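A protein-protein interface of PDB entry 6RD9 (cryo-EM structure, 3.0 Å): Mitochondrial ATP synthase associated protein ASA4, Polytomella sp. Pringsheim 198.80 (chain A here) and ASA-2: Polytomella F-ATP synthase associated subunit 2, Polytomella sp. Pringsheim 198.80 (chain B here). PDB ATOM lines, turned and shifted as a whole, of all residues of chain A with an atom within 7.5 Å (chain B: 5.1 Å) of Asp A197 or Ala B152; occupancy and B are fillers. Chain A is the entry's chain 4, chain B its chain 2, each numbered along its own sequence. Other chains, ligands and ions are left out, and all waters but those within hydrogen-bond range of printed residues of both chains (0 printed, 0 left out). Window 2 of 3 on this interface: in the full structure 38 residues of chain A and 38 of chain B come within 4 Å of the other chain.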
ATOM      1  N   SER A 190     -14.710  25.303  26.236  1.00  0.00           N
ATOM      2  CA  SER A 190     -14.381  26.462  25.420  1.00  0.00           C
ATOM      3  C   SER A 190     -14.541  26.090  23.955  1.00  0.00           C
ATOM      4  O   SER A 190     -14.707  24.921  23.601  1.00  0.00           O
ATOM      5  CB  SER A 190     -12.967  26.975  25.690  1.00  0.00           C
ATOM      6  OG  SER A 190     -12.683  28.088  24.864  1.00  0.00           O
ATOM      7  N   ASN A 192     -12.384  26.934  21.035  1.00  0.00           N
ATOM      8  CA  ASN A 192     -11.180  26.412  20.414  1.00  0.00           C
ATOM      9  C   ASN A 192     -10.626  25.244  21.212  1.00  0.00           C
ATOM     10  O   ASN A 192     -10.729  25.197  22.438  1.00  0.00           O
ATOM     11  CB  ASN A 192     -10.124  27.503  20.306  1.00  0.00           C
ATOM     12  CG  ASN A 192     -10.064  28.362  21.541  1.00  0.00           C
ATOM     13  OD1 ASN A 192     -10.838  28.168  22.474  1.00  0.00           O
ATOM     14  ND2 ASN A 192      -9.154  29.324  21.555  1.00  0.00           N
ATOM     15  N   GLU A 193     -10.023  24.297  20.500  1.00  0.00           N
ATOM     16  CA  GLU A 193      -9.460  23.138  21.168  1.00  0.00           C
ATOM     17  C   GLU A 193      -8.106  23.430  21.792  1.00  0.00           C
ATOM     18  O   GLU A 193      -7.596  22.594  22.539  1.00  0.00           O
ATOM     19  CB  GLU A 193      -9.330  21.970  20.195  1.00  0.00           C
ATOM     20  CG  GLU A 193      -8.199  22.099  19.204  1.00  0.00           C
ATOM     21  CD  GLU A 193      -8.106  20.895  18.292  1.00  0.00           C
ATOM     22  OE1 GLU A 193      -8.091  21.076  17.056  1.00  0.00           O
ATOM     23  OE2 GLU A 193      -8.053  19.764  18.811  1.00  0.00           O
ATOM     24  N   ASP A 194      -7.511  24.582  21.499  1.00  0.00           N
ATOM     25  CA  ASP A 194      -6.240  24.938  22.105  1.00  0.00           C
ATOM     26  C   ASP A 194      -6.393  25.666  23.427  1.00  0.00           C
ATOM     27  O   ASP A 194      -5.561  25.485  24.313  1.00  0.00           O
ATOM     28  CB  ASP A 194      -5.413  25.787  21.145  1.00  0.00           C
ATOM     29  CG  ASP A 194      -4.835  24.974  20.013  1.00  0.00           C
ATOM     30  OD1 ASP A 194      -4.560  23.778  20.232  1.00  0.00           O
ATOM     31  OD2 ASP A 194      -4.657  25.523  18.907  1.00  0.00           O
ATOM     32  N   ALA A 195      -7.421  26.484  23.595  1.00  0.00           N
ATOM     33  CA  ALA A 195      -7.604  27.126  24.887  1.00  0.00           C
ATOM     34  C   ALA A 195      -8.334  26.241  25.877  1.00  0.00           C
ATOM     35  O   ALA A 195      -8.274  26.511  27.079  1.00  0.00           O
ATOM     36  CB  ALA A 195      -8.363  28.442  24.735  1.00  0.00           C
ATOM     37  N   ALA A 196      -9.033  25.209  25.407  1.00  0.00           N
ATOM     38  CA  ALA A 196      -9.589  24.208  26.304  1.00  0.00           C
ATOM     39  C   ALA A 196      -8.576  23.137  26.664  1.00  0.00           C
ATOM     40  O   ALA A 196      -8.789  22.403  27.631  1.00  0.00           O
ATOM     41  CB  ALA A 196     -10.822  23.558  25.681  1.00  0.00           C
ATOM     42  N   ASP A 197      -7.480  23.043  25.918  1.00  0.00           N
ATOM     43  CA  ASP A 197      -6.413  22.111  26.244  1.00  0.00           C
ATOM     44  C   ASP A 197      -5.616  22.593  27.442  1.00  0.00           C
ATOM     45  O   ASP A 197      -5.157  21.788  28.251  1.00  0.00           O
ATOM     46  CB  ASP A 197      -5.500  21.936  25.039  1.00  0.00           C
ATOM     47  CG  ASP A 197      -4.334  21.017  25.313  1.00  0.00           C
ATOM     48  OD1 ASP A 197      -4.496  19.793  25.150  1.00  0.00           O
ATOM     49  OD2 ASP A 197      -3.249  21.514  25.675  1.00  0.00           O
ATOM     50  N   LYS A 198      -5.417  23.898  27.557  1.00  0.00           N
ATOM     51  CA  LYS A 198      -4.671  24.420  28.688  1.00  0.00           C
ATOM     52  C   LYS A 198      -5.486  24.439  29.964  1.00  0.00           C
ATOM     53  O   LYS A 198      -4.900  24.542  31.043  1.00  0.00           O
ATOM     54  CB  LYS A 198      -4.163  25.837  28.412  1.00  0.00           C
ATOM     55  CG  LYS A 198      -2.820  25.932  27.690  1.00  0.00           C
ATOM     56  CD  LYS A 198      -2.943  25.666  26.209  1.00  0.00           C
ATOM     57  CE  LYS A 198      -1.630  25.849  25.480  1.00  0.00           C
ATOM     58  NZ  LYS A 198      -1.744  25.499  24.037  1.00  0.00           N
ATOM     59  N   VAL A 199      -6.808  24.347  29.878  1.00  0.00           N
ATOM     60  CA  VAL A 199      -7.608  24.290  31.089  1.00  0.00           C
ATOM     61  C   VAL A 199      -7.858  22.843  31.504  1.00  0.00           C
ATOM     62  O   VAL A 199      -8.141  22.573  32.673  1.00  0.00           O
ATOM     63  CB  VAL A 199      -8.921  25.073  30.907  1.00  0.00           C
ATOM     64  CG1 VAL A 199      -9.922  24.312  30.073  1.00  0.00           C
ATOM     65  CG2 VAL A 199      -9.505  25.471  32.232  1.00  0.00           C
ATOM     66  N   SER A 200      -7.718  21.889  30.580  1.00  0.00           N
ATOM     67  CA  SER A 200      -7.810  20.495  30.977  1.00  0.00           C
ATOM     68  C   SER A 200      -6.530  20.039  31.643  1.00  0.00           C
ATOM     69  O   SER A 200      -6.574  19.214  32.553  1.00  0.00           O
ATOM     70  CB  SER A 200      -8.096  19.596  29.785  1.00  0.00           C
ATOM     71  OG  SER A 200      -6.930  19.431  29.013  1.00  0.00           O
ATOM     72  N   LYS A 201      -5.393  20.583  31.229  1.00  0.00           N
ATOM     73  CA  LYS A 201      -4.129  20.256  31.863  1.00  0.00           C
ATOM     74  C   LYS A 201      -3.970  20.869  33.239  1.00  0.00           C
ATOM     75  O   LYS A 201      -3.047  20.483  33.956  1.00  0.00           O
ATOM     76  CB  LYS A 201      -2.962  20.708  31.001  1.00  0.00           C
ATOM     77  CG  LYS A 201      -2.726  19.860  29.785  1.00  0.00           C
ATOM     78  CD  LYS A 201      -1.799  20.563  28.839  1.00  0.00           C
ATOM     79  CE  LYS A 201      -0.502  20.944  29.513  1.00  0.00           C
ATOM     80  NZ  LYS A 201       0.289  19.757  29.894  1.00  0.00           N
ATOM     81  N   GLU A 202      -4.802  21.827  33.624  1.00  0.00           N
ATOM     82  CA  GLU A 202      -4.766  22.321  34.985  1.00  0.00           C
ATOM     83  C   GLU A 202      -5.995  21.948  35.786  1.00  0.00           C
ATOM     84  O   GLU A 202      -6.028  22.212  36.988  1.00  0.00           O
ATOM     85  CB  GLU A 202      -4.579  23.842  35.018  1.00  0.00           C
ATOM     86  CG  GLU A 202      -5.620  24.622  34.276  1.00  0.00           C
ATOM     87  CD  GLU A 202      -5.290  26.095  34.207  1.00  0.00           C
ATOM     88  OE1 GLU A 202      -5.954  26.816  33.432  1.00  0.00           O
ATOM     89  OE2 GLU A 202      -4.372  26.534  34.929  1.00  0.00           O
ATOM     90  N   PHE A 203      -7.014  21.378  35.149  1.00  0.00           N
ATOM     91  CA  PHE A 203      -8.012  20.638  35.908  1.00  0.00           C
ATOM     92  C   PHE A 203      -7.452  19.298  36.347  1.00  0.00           C
ATOM     93  O   PHE A 203      -7.571  18.919  37.517  1.00  0.00           O
ATOM     94  CB  PHE A 203      -9.263  20.426  35.075  1.00  0.00           C
ATOM     95  CG  PHE A 203     -10.249  19.499  35.700  1.00  0.00           C
ATOM     96  CD1 PHE A 203     -11.018  19.909  36.758  1.00  0.00           C
ATOM     97  CD2 PHE A 203     -10.421  18.225  35.215  1.00  0.00           C
ATOM     98  CE1 PHE A 203     -11.931  19.066  37.319  1.00  0.00           C
ATOM     99  CE2 PHE A 203     -11.329  17.379  35.783  1.00  0.00           C
ATOM    100  CZ  PHE A 203     -12.082  17.803  36.833  1.00  0.00           C
ATOM    101  N   PHE A 204      -6.824  18.574  35.423  1.00  0.00           N
ATOM    102  CA  PHE A 204      -6.247  17.279  35.740  1.00  0.00           C
ATOM    103  C   PHE A 204      -5.029  17.388  36.630  1.00  0.00           C
ATOM    104  O   PHE A 204      -4.615  16.386  37.205  1.00  0.00           O
ATOM    105  CB  PHE A 204      -5.893  16.546  34.458  1.00  0.00           C
ATOM    106  CG  PHE A 204      -7.080  16.018  33.732  1.00  0.00           C
ATOM    107  CD1 PHE A 204      -7.077  15.921  32.365  1.00  0.00           C
ATOM    108  CD2 PHE A 204      -8.199  15.615  34.420  1.00  0.00           C
ATOM    109  CE1 PHE A 204      -8.171  15.435  31.700  1.00  0.00           C
ATOM    110  CE2 PHE A 204      -9.294  15.131  33.759  1.00  0.00           C
ATOM    111  CZ  PHE A 204      -9.279  15.042  32.403  1.00  0.00           C
ATOM    112  N   VAL B 125       7.706  19.603  24.262  1.00  0.00           N
ATOM    113  CA  VAL B 125       7.431  20.806  23.484  1.00  0.00           C
ATOM    114  C   VAL B 125       8.362  21.963  23.842  1.00  0.00           C
ATOM    115  O   VAL B 125       8.482  22.908  23.050  1.00  0.00           O
ATOM    116  CB  VAL B 125       5.957  21.246  23.610  1.00  0.00           C
ATOM    117  CG1 VAL B 125       5.039  20.105  23.258  1.00  0.00           C
ATOM    118  CG2 VAL B 125       5.655  21.766  24.988  1.00  0.00           C
ATOM    119  N   ASN B 149      -5.686  13.647  27.014  1.00  0.00           N
ATOM    120  CA  ASN B 149      -6.025  14.139  25.682  1.00  0.00           C
ATOM    121  C   ASN B 149      -5.265  15.429  25.392  1.00  0.00           C
ATOM    122  O   ASN B 149      -5.834  16.500  25.215  1.00  0.00           O
ATOM    123  CB  ASN B 149      -7.526  14.342  25.551  1.00  0.00           C
ATOM    124  CG  ASN B 149      -7.982  14.295  24.117  1.00  0.00           C
ATOM    125  OD1 ASN B 149      -7.937  15.294  23.407  1.00  0.00           O
ATOM    126  ND2 ASN B 149      -8.424  13.126  23.678  1.00  0.00           N
ATOM    127  N   ASP B 150      -3.944  15.302  25.361  1.00  0.00           N
ATOM    128  CA  ASP B 150      -3.071  16.448  25.167  1.00  0.00           C
ATOM    129  C   ASP B 150      -3.008  16.747  23.684  1.00  0.00           C
ATOM    130  O   ASP B 150      -2.265  16.093  22.948  1.00  0.00           O
ATOM    131  CB  ASP B 150      -1.678  16.170  25.713  1.00  0.00           C
ATOM    132  CG  ASP B 150      -1.012  17.410  26.237  1.00  0.00           C
ATOM    133  OD1 ASP B 150      -1.707  18.424  26.399  1.00  0.00           O
ATOM    134  OD2 ASP B 150       0.201  17.381  26.482  1.00  0.00           O
ATOM    135  N   VAL B 151      -3.789  17.731  23.237  1.00  0.00           N
ATOM    136  CA  VAL B 151      -3.733  18.120  21.836  1.00  0.00           C
ATOM    137  C   VAL B 151      -2.655  19.152  21.579  1.00  0.00           C
ATOM    138  O   VAL B 151      -2.375  19.452  20.414  1.00  0.00           O
ATOM    139  CB  VAL B 151      -5.079  18.668  21.333  1.00  0.00           C
ATOM    140  CG1 VAL B 151      -6.186  17.671  21.608  1.00  0.00           C
ATOM    141  CG2 VAL B 151      -5.374  19.995  21.952  1.00  0.00           C
ATOM    142  N   ALA B 152      -2.045  19.710  22.624  1.00  0.00           N
ATOM    143  CA  ALA B 152      -0.889  20.572  22.422  1.00  0.00           C
ATOM    144  C   ALA B 152       0.292  19.778  21.897  1.00  0.00           C
ATOM    145  O   ALA B 152       1.045  20.262  21.050  1.00  0.00           O
ATOM    146  CB  ALA B 152      -0.521  21.273  23.722  1.00  0.00           C
ATOM    147  N   LEU B 153       0.460  18.552  22.378  1.00  0.00           N
ATOM    148  CA  LEU B 153       1.511  17.692  21.856  1.00  0.00           C
ATOM    149  C   LEU B 153       1.146  17.143  20.489  1.00  0.00           C
ATOM    150  O   LEU B 153       2.024  16.980  19.638  1.00  0.00           O
ATOM    151  CB  LEU B 153       1.785  16.563  22.845  1.00  0.00           C
ATOM    152  CG  LEU B 153       2.424  15.258  22.377  1.00  0.00           C
ATOM    153  CD1 LEU B 153       3.863  15.474  22.029  1.00  0.00           C
ATOM    154  CD2 LEU B 153       2.288  14.206  23.434  1.00  0.00           C
ATOM    155  N   ALA B 154      -0.136  16.872  20.250  1.00  0.00           N
ATOM    156  CA  ALA B 154      -0.548  16.286  18.980  1.00  0.00           C
ATOM    157  C   ALA B 154      -0.433  17.283  17.838  1.00  0.00           C
ATOM    158  O   ALA B 154      -0.340  16.887  16.673  1.00  0.00           O
ATOM    159  CB  ALA B 154      -1.974  15.762  19.084  1.00  0.00           C
ATOM    160  N   LYS B 155      -0.445  18.575  18.151  1.00  0.00           N
ATOM    161  CA  LYS B 155      -0.132  19.581  17.152  1.00  0.00           C
ATOM    162  C   LYS B 155       1.369  19.689  16.938  1.00  0.00           C
ATOM    163  O   LYS B 155       1.832  19.714  15.794  1.00  0.00           O
ATOM    164  CB  LYS B 155      -0.717  20.921  17.577  1.00  0.00           C
ATOM    165  CG  LYS B 155      -2.212  20.929  17.496  1.00  0.00           C
ATOM    166  CD  LYS B 155      -2.782  22.300  17.679  1.00  0.00           C
ATOM    167  CE  LYS B 155      -4.245  22.289  17.296  1.00  0.00           C
ATOM    168  NZ  LYS B 155      -4.774  23.655  17.090  1.00  0.00           N
ATOM    169  N   ALA B 156       2.141  19.721  18.026  1.00  0.00           N
ATOM    170  CA  ALA B 156       3.590  19.818  17.913  1.00  0.00           C
ATOM    171  C   ALA B 156       4.197  18.565  17.307  1.00  0.00           C
ATOM    172  O   ALA B 156       5.249  18.637  16.669  1.00  0.00           O
ATOM    173  CB  ALA B 156       4.204  20.089  19.282  1.00  0.00           C
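Glu A193 touches Val B151. Asn B149 touches Asp A197. OD2 of Asp A197 touches CB of Ala B152 (3.4 Å). CD of Lys A201 touches OD1 of Asp B150, 3.2 Å away.
The side-chain carboxylate of Asp A197 sits close to the side-chain carboxylate of Asp B150, at 3.3 Å. The side-chain carboxylate (OD2) of Asp A194 lies within salt-bridge range of the side-chain amino group (NZ) of Lys B155 (2.6 Å). The side-chain carboxylate of Asp A197 sits at hydrogen-bond distance from the backbone NH of Val B151.
Of chain B, only Asn B149 (3.6 Å), Asp B150 (3.3 Å), Val B151 (2.9 Å) and Ala B152 (3.4 Å) come within 4 Å of Asp A197. Of the printed residues of chain A, Val B151 touches Glu A193 and Asp A197. Of the printed residues of chain A, Asp B150 touches Asp A197 and Lys A201. Printed residues of chain A within 4 Å of Asn B149: Asp A197. Of the printed residues of chain B, Glu A193 touches Val B151 (3.5 Å). Ala B156 touches none of the printed residues of chain A. The nearest printed residue of chain B that does not touch Asp A197 is Leu B153 (5.8 Å). The nearest residue of chain A that does not touch Ala B152 is Lys A198 (4.4 Å).
Of the 9 printed residues of chain B, 5 touch a printed residue of chain A. Printed residues of chain B that touch a printed residue of chain A: Asn B149, Asp B150, Val B151, Ala B152 and Lys B155. Hydrophobic or aromatic side chains of chain B within 4 Å of the printed part of chain A: Val B151 and Ala B152. Of the 14 printed residues of chain A, 4 touch a printed residue of chain B. Among the printed residues, Asp or Glu carboxylates within 4 Å of a Lys or Arg side-chain nitrogen of the other chain: Asp A194 with Lys B155 (2.6 Å).
O of Asp A197 lies within hydrogen-bond range of OG of Ser A200 (3.0 Å).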
